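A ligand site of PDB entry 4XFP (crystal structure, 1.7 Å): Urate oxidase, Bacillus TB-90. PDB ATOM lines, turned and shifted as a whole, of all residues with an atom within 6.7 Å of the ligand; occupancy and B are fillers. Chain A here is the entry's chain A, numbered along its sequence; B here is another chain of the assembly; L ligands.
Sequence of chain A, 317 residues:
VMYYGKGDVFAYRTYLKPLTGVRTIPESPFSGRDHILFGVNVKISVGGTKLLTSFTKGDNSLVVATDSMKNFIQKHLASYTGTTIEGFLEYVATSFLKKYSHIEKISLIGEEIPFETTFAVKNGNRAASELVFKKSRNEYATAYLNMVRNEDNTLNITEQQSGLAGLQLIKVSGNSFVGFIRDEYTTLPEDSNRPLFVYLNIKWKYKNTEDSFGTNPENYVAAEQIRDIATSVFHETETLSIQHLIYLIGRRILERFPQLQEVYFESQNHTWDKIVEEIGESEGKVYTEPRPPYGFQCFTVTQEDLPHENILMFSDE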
ATOM      1  N   SER A 176      14.736 -31.504   1.707  1.00  0.00           N
ATOM      2  CA  SER A 176      15.290 -30.444   2.534  1.00  0.00           C
ATOM      3  C   SER A 176      16.734 -30.139   2.145  1.00  0.00           C
ATOM      4  O   SER A 176      17.419 -30.955   1.529  1.00  0.00           O
ATOM      5  CB  SER A 176      15.227 -30.817   4.020  1.00  0.00           C
ATOM      6  OG  SER A 176      16.274 -31.699   4.370  1.00  0.00           O
ATOM      7  N   PHE A 177      17.173 -28.949   2.507  1.00  0.00           N
ATOM      8  CA  PHE A 177      18.587 -28.624   2.449  1.00  0.00           C
ATOM      9  C   PHE A 177      18.887 -27.757   3.658  1.00  0.00           C
ATOM     10  O   PHE A 177      18.591 -26.569   3.670  1.00  0.00           O
ATOM     11  CB  PHE A 177      18.972 -27.925   1.146  1.00  0.00           C
ATOM     12  CG  PHE A 177      20.456 -27.761   0.995  1.00  0.00           C
ATOM     13  CD1 PHE A 177      21.284 -28.872   0.976  1.00  0.00           C
ATOM     14  CD2 PHE A 177      21.024 -26.499   0.895  1.00  0.00           C
ATOM     15  CE1 PHE A 177      22.653 -28.728   0.851  1.00  0.00           C
ATOM     16  CE2 PHE A 177      22.396 -26.360   0.762  1.00  0.00           C
ATOM     17  CZ  PHE A 177      23.211 -27.474   0.740  1.00  0.00           C
ATOM     18  N   PHE A 180      24.072 -26.837   6.277  1.00  0.00           N
ATOM     19  CA  PHE A 180      25.261 -26.439   5.538  1.00  0.00           C
ATOM     20  C   PHE A 180      25.980 -25.287   6.238  1.00  0.00           C
ATOM     21  O   PHE A 180      25.447 -24.658   7.146  1.00  0.00           O
ATOM     22  CB  PHE A 180      24.889 -26.051   4.103  1.00  0.00           C
ATOM     23  CG  PHE A 180      23.775 -25.052   4.005  1.00  0.00           C
ATOM     24  CD1 PHE A 180      22.460 -25.477   3.905  1.00  0.00           C
ATOM     25  CD2 PHE A 180      24.034 -23.701   4.004  1.00  0.00           C
ATOM     26  CE1 PHE A 180      21.429 -24.557   3.805  1.00  0.00           C
ATOM     27  CE2 PHE A 180      23.010 -22.785   3.910  1.00  0.00           C
ATOM     28  CZ  PHE A 180      21.703 -23.214   3.816  1.00  0.00           C
ATOM     29  N   LEU A 188      21.999 -17.945   2.071  1.00  0.00           N
ATOM     30  CA  LEU A 188      20.955 -18.920   1.761  1.00  0.00           C
ATOM     31  C   LEU A 188      20.198 -19.382   3.012  1.00  0.00           C
ATOM     32  O   LEU A 188      20.809 -19.901   3.950  1.00  0.00           O
ATOM     33  CB  LEU A 188      21.573 -20.140   1.059  1.00  0.00           C
ATOM     34  CG  LEU A 188      20.620 -21.259   0.641  1.00  0.00           C
ATOM     35  CD1 LEU A 188      19.663 -20.791  -0.454  1.00  0.00           C
ATOM     36  CD2 LEU A 188      21.400 -22.502   0.192  1.00  0.00           C
ATOM     37  N   ARG A 194      11.564 -28.000   0.177  1.00  0.00           N
ATOM     38  CA  ARG A 194      11.719 -27.293  -1.092  1.00  0.00           C
ATOM     39  C   ARG A 194      11.216 -28.174  -2.229  1.00  0.00           C
ATOM     40  O   ARG A 194      11.245 -29.406  -2.127  1.00  0.00           O
ATOM     41  CB  ARG A 194      13.183 -26.914  -1.316  1.00  0.00           C
ATOM     42  CG  ARG A 194      14.109 -28.113  -1.501  1.00  0.00           C
ATOM     43  CD  ARG A 194      15.541 -27.658  -1.686  1.00  0.00           C
ATOM     44  NE  ARG A 194      16.433 -28.806  -1.792  1.00  0.00           N
ATOM     45  CZ  ARG A 194      17.707 -28.709  -2.145  1.00  0.00           C
ATOM     46  NH1 ARG A 194      18.210 -27.522  -2.441  1.00  0.00           N
ATOM     47  NH2 ARG A 194      18.465 -29.804  -2.205  1.00  0.00           N
ATOM     48  N   LEU A 196      12.409 -29.484  -4.959  1.00  0.00           N
ATOM     49  CA  LEU A 196      13.683 -29.727  -5.612  1.00  0.00           C
ATOM     50  C   LEU A 196      13.529 -30.057  -7.094  1.00  0.00           C
ATOM     51  O   LEU A 196      12.815 -31.006  -7.453  1.00  0.00           O
ATOM     52  CB  LEU A 196      14.420 -30.873  -4.911  1.00  0.00           C
ATOM     53  CG  LEU A 196      15.758 -31.271  -5.524  1.00  0.00           C
ATOM     54  CD1 LEU A 196      16.730 -30.098  -5.565  1.00  0.00           C
ATOM     55  CD2 LEU A 196      16.338 -32.418  -4.713  1.00  0.00           C
ATOM     56  N   LEU A 240      18.026 -35.022   1.224  1.00  0.00           N
ATOM     57  CA  LEU A 240      18.747 -34.137   2.124  1.00  0.00           C
ATOM     58  C   LEU A 240      19.652 -33.171   1.361  1.00  0.00           C
ATOM     59  O   LEU A 240      20.182 -32.212   1.925  1.00  0.00           O
ATOM     60  CB  LEU A 240      19.554 -34.972   3.125  1.00  0.00           C
ATOM     61  CG  LEU A 240      18.718 -35.850   4.052  1.00  0.00           C
ATOM     62  CD1 LEU A 240      19.599 -36.798   4.829  1.00  0.00           C
ATOM     63  CD2 LEU A 240      17.899 -34.972   5.002  1.00  0.00           C
ATOM     64  N   SER A 241      19.790 -33.441   0.059  1.00  0.00           N
ATOM     65  CA  SER A 241      20.565 -32.641  -0.896  1.00  0.00           C
ATOM     66  C   SER A 241      20.512 -33.379  -2.207  1.00  0.00           C
ATOM     67  O   SER A 241      20.094 -34.529  -2.254  1.00  0.00           O
ATOM     68  CB  SER A 241      22.019 -32.472  -0.465  1.00  0.00           C
ATOM     69  OG  SER A 241      22.628 -33.746  -0.424  1.00  0.00           O
ATOM     70  N   ILE A 242      20.974 -32.734  -3.275  1.00  0.00           N
ATOM     71  CA  ILE A 242      21.079 -33.415  -4.554  1.00  0.00           C
ATOM     72  C   ILE A 242      22.176 -34.497  -4.473  1.00  0.00           C
ATOM     73  O   ILE A 242      22.026 -35.589  -5.011  1.00  0.00           O
ATOM     74  CB  ILE A 242      21.373 -32.428  -5.702  1.00  0.00           C
ATOM     75  CG1 ILE A 242      20.170 -31.515  -5.923  1.00  0.00           C
ATOM     76  CG2 ILE A 242      21.671 -33.181  -6.976  1.00  0.00           C
ATOM     77  CD1 ILE A 242      20.493 -30.289  -6.770  1.00  0.00           C
ATOM     78  N   GLN A 243      23.266 -34.170  -3.772  1.00  0.00           N
ATOM     79  CA  GLN A 243      24.356 -35.089  -3.519  1.00  0.00           C
ATOM     80  C   GLN A 243      23.829 -36.419  -2.938  1.00  0.00           C
ATOM     81  O   GLN A 243      24.172 -37.497  -3.408  1.00  0.00           O
ATOM     82  CB  GLN A 243      25.365 -34.458  -2.543  1.00  0.00           C
ATOM     83  CG  GLN A 243      26.180 -33.288  -3.123  1.00  0.00           C
ATOM     84  CD  GLN A 243      25.550 -31.921  -2.916  1.00  0.00           C
ATOM     85  OE1 GLN A 243      24.339 -31.748  -3.054  1.00  0.00           O
ATOM     86  NE2 GLN A 243      26.373 -30.924  -2.629  1.00  0.00           N
ATOM     87  N   HIS A 244      22.979 -36.292  -1.920  1.00  0.00           N
ATOM     88  CA  HIS A 244      22.355 -37.425  -1.242  1.00  0.00           C
ATOM     89  C   HIS A 244      21.481 -38.223  -2.203  1.00  0.00           C
ATOM     90  O   HIS A 244      21.574 -39.451  -2.266  1.00  0.00           O
ATOM     91  CB  HIS A 244      21.537 -36.868  -0.058  1.00  0.00           C
ATOM     92  CG  HIS A 244      20.712 -37.877   0.680  1.00  0.00           C
ATOM     93  ND1 HIS A 244      19.341 -37.764   0.790  1.00  0.00           N
ATOM     94  CD2 HIS A 244      21.057 -38.971   1.404  1.00  0.00           C
ATOM     95  CE1 HIS A 244      18.875 -38.756   1.522  1.00  0.00           C
ATOM     96  NE2 HIS A 244      19.897 -39.502   1.911  1.00  0.00           N
ATOM     97  N   ASN A 269      21.049 -28.050 -10.245  1.00  0.00           N
ATOM     98  CA  ASN A 269      19.966 -27.565  -9.422  1.00  0.00           C
ATOM     99  C   ASN A 269      19.291 -26.371 -10.064  1.00  0.00           C
ATOM    100  O   ASN A 269      19.932 -25.342 -10.311  1.00  0.00           O
ATOM    101  CB  ASN A 269      20.501 -27.182  -8.036  1.00  0.00           C
ATOM    102  CG  ASN A 269      19.391 -26.949  -7.037  1.00  0.00           C
ATOM    103  OD1 ASN A 269      18.223 -26.772  -7.400  1.00  0.00           O
ATOM    104  ND2 ASN A 269      19.744 -26.925  -5.752  1.00  0.00           N
ATOM    105  N   GLY A 295      23.568 -24.589  -9.349  1.00  0.00           N
ATOM    106  CA  GLY A 295      24.459 -25.500  -8.681  1.00  0.00           C
ATOM    107  C   GLY A 295      24.604 -26.764  -9.499  1.00  0.00           C
ATOM    108  O   GLY A 295      23.700 -27.118 -10.278  1.00  0.00           O
ATOM    109  N   PHE A 296      25.722 -27.450  -9.348  1.00  0.00           N
ATOM    110  CA  PHE A 296      25.875 -28.734  -9.997  1.00  0.00           C
ATOM    111  C   PHE A 296      26.679 -29.691  -9.147  1.00  0.00           C
ATOM    112  O   PHE A 296      27.434 -29.282  -8.265  1.00  0.00           O
ATOM    113  CB  PHE A 296      26.525 -28.579 -11.376  1.00  0.00           C
ATOM    114  CG  PHE A 296      27.931 -28.039 -11.348  1.00  0.00           C
ATOM    115  CD1 PHE A 296      29.017 -28.876 -11.138  1.00  0.00           C
ATOM    116  CD2 PHE A 296      28.169 -26.691 -11.585  1.00  0.00           C
ATOM    117  CE1 PHE A 296      30.308 -28.369 -11.127  1.00  0.00           C
ATOM    118  CE2 PHE A 296      29.458 -26.196 -11.580  1.00  0.00           C
ATOM    119  CZ  PHE A 296      30.527 -27.026 -11.344  1.00  0.00           C
ATOM    120  N   GLN A 297      26.504 -30.973  -9.433  1.00  0.00           N
ATOM    121  CA  GLN A 297      27.142 -32.045  -8.696  1.00  0.00           C
ATOM    122  C   GLN A 297      27.596 -33.104  -9.677  1.00  0.00           C
ATOM    123  O   GLN A 297      26.950 -33.352 -10.691  1.00  0.00           O
ATOM    124  CB  GLN A 297      26.181 -32.651  -7.670  1.00  0.00           C
ATOM    125  CG  GLN A 297      25.679 -31.706  -6.586  1.00  0.00           C
ATOM    126  CD  GLN A 297      24.619 -30.720  -7.059  1.00  0.00           C
ATOM    127  OE1 GLN A 297      23.925 -30.951  -8.054  1.00  0.00           O
ATOM    128  NE2 GLN A 297      24.505 -29.604  -6.347  1.00  0.00           N
ATOM    129  N   TYR B   4      31.504 -30.663  -6.805  1.00  0.00           N
ATOM    130  CA  TYR B   4      30.266 -29.915  -6.972  1.00  0.00           C
ATOM    131  C   TYR B   4      30.622 -28.443  -7.099  1.00  0.00           C
ATOM    132  O   TYR B   4      31.776 -28.056  -6.892  1.00  0.00           O
ATOM    133  CB  TYR B   4      29.286 -30.178  -5.810  1.00  0.00           C
ATOM    134  CG  TYR B   4      29.572 -29.446  -4.519  1.00  0.00           C
ATOM    135  CD1 TYR B   4      30.748 -29.647  -3.831  1.00  0.00           C
ATOM    136  CD2 TYR B   4      28.627 -28.590  -3.966  1.00  0.00           C
ATOM    137  CE1 TYR B   4      31.007 -29.002  -2.635  1.00  0.00           C
ATOM    138  CE2 TYR B   4      28.874 -27.925  -2.776  1.00  0.00           C
ATOM    139  CZ  TYR B   4      30.070 -28.138  -2.122  1.00  0.00           C
ATOM    140  OH  TYR B   4      30.356 -27.492  -0.941  1.00  0.00           O
ATOM    141  N   GLY B   5      29.668 -27.619  -7.484  1.00  0.00           N
ATOM    142  CA  GLY B   5      29.979 -26.232  -7.664  1.00  0.00           C
ATOM    143  C   GLY B   5      28.849 -25.411  -8.213  1.00  0.00           C
ATOM    144  O   GLY B   5      27.678 -25.768  -8.065  1.00  0.00           O
ATOM    145  N   LYS B   6      29.198 -24.294  -8.837  1.00  0.00           N
ATOM    146  CA  LYS B   6      28.210 -23.354  -9.362  1.00  0.00           C
ATOM    147  C   LYS B   6      28.613 -22.922 -10.763  1.00  0.00           C
ATOM    148  O   LYS B   6      29.762 -22.583 -10.985  1.00  0.00           O
ATOM    149  CB  LYS B   6      28.103 -22.126  -8.478  1.00  0.00           C
ATOM    150  CG  LYS B   6      26.815 -21.334  -8.672  1.00  0.00           C
ATOM    151  CD  LYS B   6      25.687 -21.965  -7.856  1.00  0.00           C
ATOM    152  CE  LYS B   6      24.488 -21.072  -7.745  1.00  0.00           C
ATOM    153  NZ  LYS B   6      23.462 -21.729  -6.881  1.00  0.00           N
ATOM    154  N   ASN B  60      25.509 -32.511   5.577  1.00  0.00           N
ATOM    155  CA  ASN B  60      25.828 -31.223   4.969  1.00  0.00           C
ATOM    156  C   ASN B  60      26.788 -30.373   5.807  1.00  0.00           C
ATOM    157  O   ASN B  60      27.058 -29.227   5.461  1.00  0.00           O
ATOM    158  CB  ASN B  60      24.548 -30.446   4.701  1.00  0.00           C
ATOM    159  CG  ASN B  60      23.708 -31.062   3.611  1.00  0.00           C
ATOM    160  OD1 ASN B  60      24.243 -31.582   2.634  1.00  0.00           O
ATOM    161  ND2 ASN B  60      22.391 -31.016   3.763  1.00  0.00           N
ATOM    162  N   VAL B  63      29.509 -28.862   3.825  1.00  0.00           N
ATOM    163  CA  VAL B  63      29.076 -28.358   2.529  1.00  0.00           C
ATOM    164  C   VAL B  63      29.025 -26.836   2.548  1.00  0.00           C
ATOM    165  O   VAL B  63      28.272 -26.235   3.313  1.00  0.00           O
ATOM    166  CB  VAL B  63      27.691 -28.908   2.136  1.00  0.00           C
ATOM    167  CG1 VAL B  63      27.185 -28.238   0.854  1.00  0.00           C
ATOM    168  CG2 VAL B  63      27.737 -30.433   1.965  1.00  0.00           C
ATOM    169  N   VAL B  64      29.879 -26.209   1.741  1.00  0.00           N
ATOM    170  CA  VAL B  64      29.723 -24.818   1.365  1.00  0.00           C
ATOM    171  C   VAL B  64      28.583 -24.779   0.366  1.00  0.00           C
ATOM    172  O   VAL B  64      28.655 -25.437  -0.663  1.00  0.00           O
ATOM    173  CB  VAL B  64      31.028 -24.224   0.753  1.00  0.00           C
ATOM    174  CG1 VAL B  64      30.847 -22.768   0.349  1.00  0.00           C
ATOM    175  CG2 VAL B  64      32.179 -24.357   1.729  1.00  0.00           C
ATOM    176  N   ALA B  65      27.518 -24.049   0.668  1.00  0.00           N
ATOM    177  CA  ALA B  65      26.378 -23.985  -0.246  1.00  0.00           C
ATOM    178  C   ALA B  65      26.850 -23.412  -1.568  1.00  0.00           C
ATOM    179  O   ALA B  65      27.730 -22.559  -1.608  1.00  0.00           O
ATOM    180  CB  ALA B  65      25.243 -23.170   0.325  1.00  0.00           C
ATOM    181  N   THR B  66      26.313 -23.906  -2.679  1.00  0.00           N
ATOM    182  CA  THR B  66      26.747 -23.397  -3.964  1.00  0.00           C
ATOM    183  C   THR B  66      26.346 -21.922  -4.095  1.00  0.00           C
ATOM    184  O   THR B  66      27.061 -21.140  -4.708  1.00  0.00           O
ATOM    185  CB  THR B  66      26.175 -24.219  -5.131  1.00  0.00           C
ATOM    186  OG1 THR B  66      24.754 -24.086  -5.171  1.00  0.00           O
ATOM    187  CG2 THR B  66      26.547 -25.691  -4.977  1.00  0.00           C
ATOM    188  N   ASP B  67      25.228 -21.552  -3.481  1.00  0.00           N
ATOM    189  CA  ASP B  67      24.830 -20.151  -3.423  1.00  0.00           C
ATOM    190  C   ASP B  67      25.907 -19.300  -2.751  1.00  0.00           C
ATOM    191  O   ASP B  67      26.152 -18.151  -3.149  1.00  0.00           O
ATOM    192  CB  ASP B  67      23.499 -19.989  -2.666  1.00  0.00           C
ATOM    193  CG  ASP B  67      22.990 -18.561  -2.675  1.00  0.00           C
ATOM    194  OD1 ASP B  67      22.419 -18.146  -3.718  1.00  0.00           O
ATOM    195  OD2 ASP B  67      23.153 -17.843  -1.658  1.00  0.00           O
ATOM    196  N   SER B  68      26.561 -19.854  -1.733  1.00  0.00           N
ATOM    197  CA  SER B  68      27.636 -19.142  -1.048  1.00  0.00           C
ATOM    198  C   SER B  68      28.863 -18.987  -1.930  1.00  0.00           C
ATOM    199  O   SER B  68      29.553 -17.970  -1.880  1.00  0.00           O
ATOM    200  CB  SER B  68      27.983 -19.862   0.261  1.00  0.00           C
ATOM    201  OG  SER B  68      26.821 -20.030   1.053  1.00  0.00           O
ATOM    202  N   MET B  69      29.144 -19.985  -2.772  1.00  0.00           N
ATOM    203  CA  MET B  69      30.212 -19.852  -3.748  1.00  0.00           C
ATOM    204  C   MET B  69      29.947 -18.696  -4.706  1.00  0.00           C
ATOM    205  O   MET B  69      30.854 -17.947  -5.060  1.00  0.00           O
ATOM    206  CB  MET B  69      30.399 -21.135  -4.561  1.00  0.00           C
ATOM    207  CG  MET B  69      30.796 -22.333  -3.747  1.00  0.00           C
ATOM    208  SD  MET B  69      30.775 -23.826  -4.756  1.00  0.00           S
ATOM    209  CE  MET B  69      30.834 -25.108  -3.502  1.00  0.00           C
HETATM  210  N1  LIG L   1      23.244 -29.150  -2.786  1.00  0.00           N
HETATM  211  C1  LIG L   1      21.890 -29.009  -2.800  1.00  0.00           C
HETATM  212  O1  LIG L   1      21.148 -29.957  -2.931  1.00  0.00           O
HETATM  213  N2  LIG L   1      21.351 -27.774  -2.659  1.00  0.00           N
HETATM  214  C2  LIG L   1      22.115 -26.681  -2.511  1.00  0.00           C
HETATM  215  C3  LIG L   1      23.449 -26.815  -2.484  1.00  0.00           C
HETATM  216  C4  LIG L   1      24.033 -28.074  -2.628  1.00  0.00           C
HETATM  217  O2  LIG L   1      25.237 -28.233  -2.629  1.00  0.00           O
HETATM  218  N3  LIG L   1      23.964 -25.577  -2.324  1.00  0.00           N
HETATM  219  N4  LIG L   1      22.964 -24.682  -2.254  1.00  0.00           N
HETATM  220  N5  LIG L   1      21.800 -25.358  -2.366  1.00  0.00           N
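Merely in contact with the ligand: Phe 177, Leu 188, Ser 241, Asn 269, Gln 297, Tyr 4 of chain B, Val 63 of chain B and Ala 65 of chain B. Hydrophobic or aromatic side chains within 4 Å of the ligand: Phe 177, Leu 188, Ile 242, Tyr 4 of chain B, Val 63 of chain B and Ala 65 of chain B.
The backbone NH (N) of Gln 243 sits close to the side-chain hydroxyl (OG) of Ser 241, 3.4 Å away. OG1 of Thr 66 of chain B is in hydrogen-bond range of NZ of Lys 6 of chain B (3.2 Å). The backbone NH of His 244 is in hydrogen-bond range of the side-chain hydroxyl of Ser 241, at 3.0 Å. The backbone NH (N) of Asn 269 sits at hydrogen-bond distance from the backbone carbonyl oxygen (O) of Gly 295, at 2.8 Å. The side-chain hydroxyl of Tyr 4 of chain B sits at hydrogen-bond distance from the backbone carbonyl oxygen of Val 64 of chain B (2.7 Å).
The guanidinium group of Arg 194 lies within hydrogen-bond range of an oxygen (O1) of the ligand, at 2.8 Å. An oxygen (O1) of the ligand is in hydrogen-bond range of the backbone NH of Ile 242. The side-chain amide oxygen (OE1) of Gln 243 sits at hydrogen-bond distance from a nitrogen (N1) of the ligand, at 2.8 Å. N3 of the ligand is in hydrogen-bond range of N of Thr 66 of chain B. The side-chain hydroxyl (OG1) of Thr 66 of chain B is in hydrogen-bond range of a nitrogen (N3) of the ligand, 3.3 Å away.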
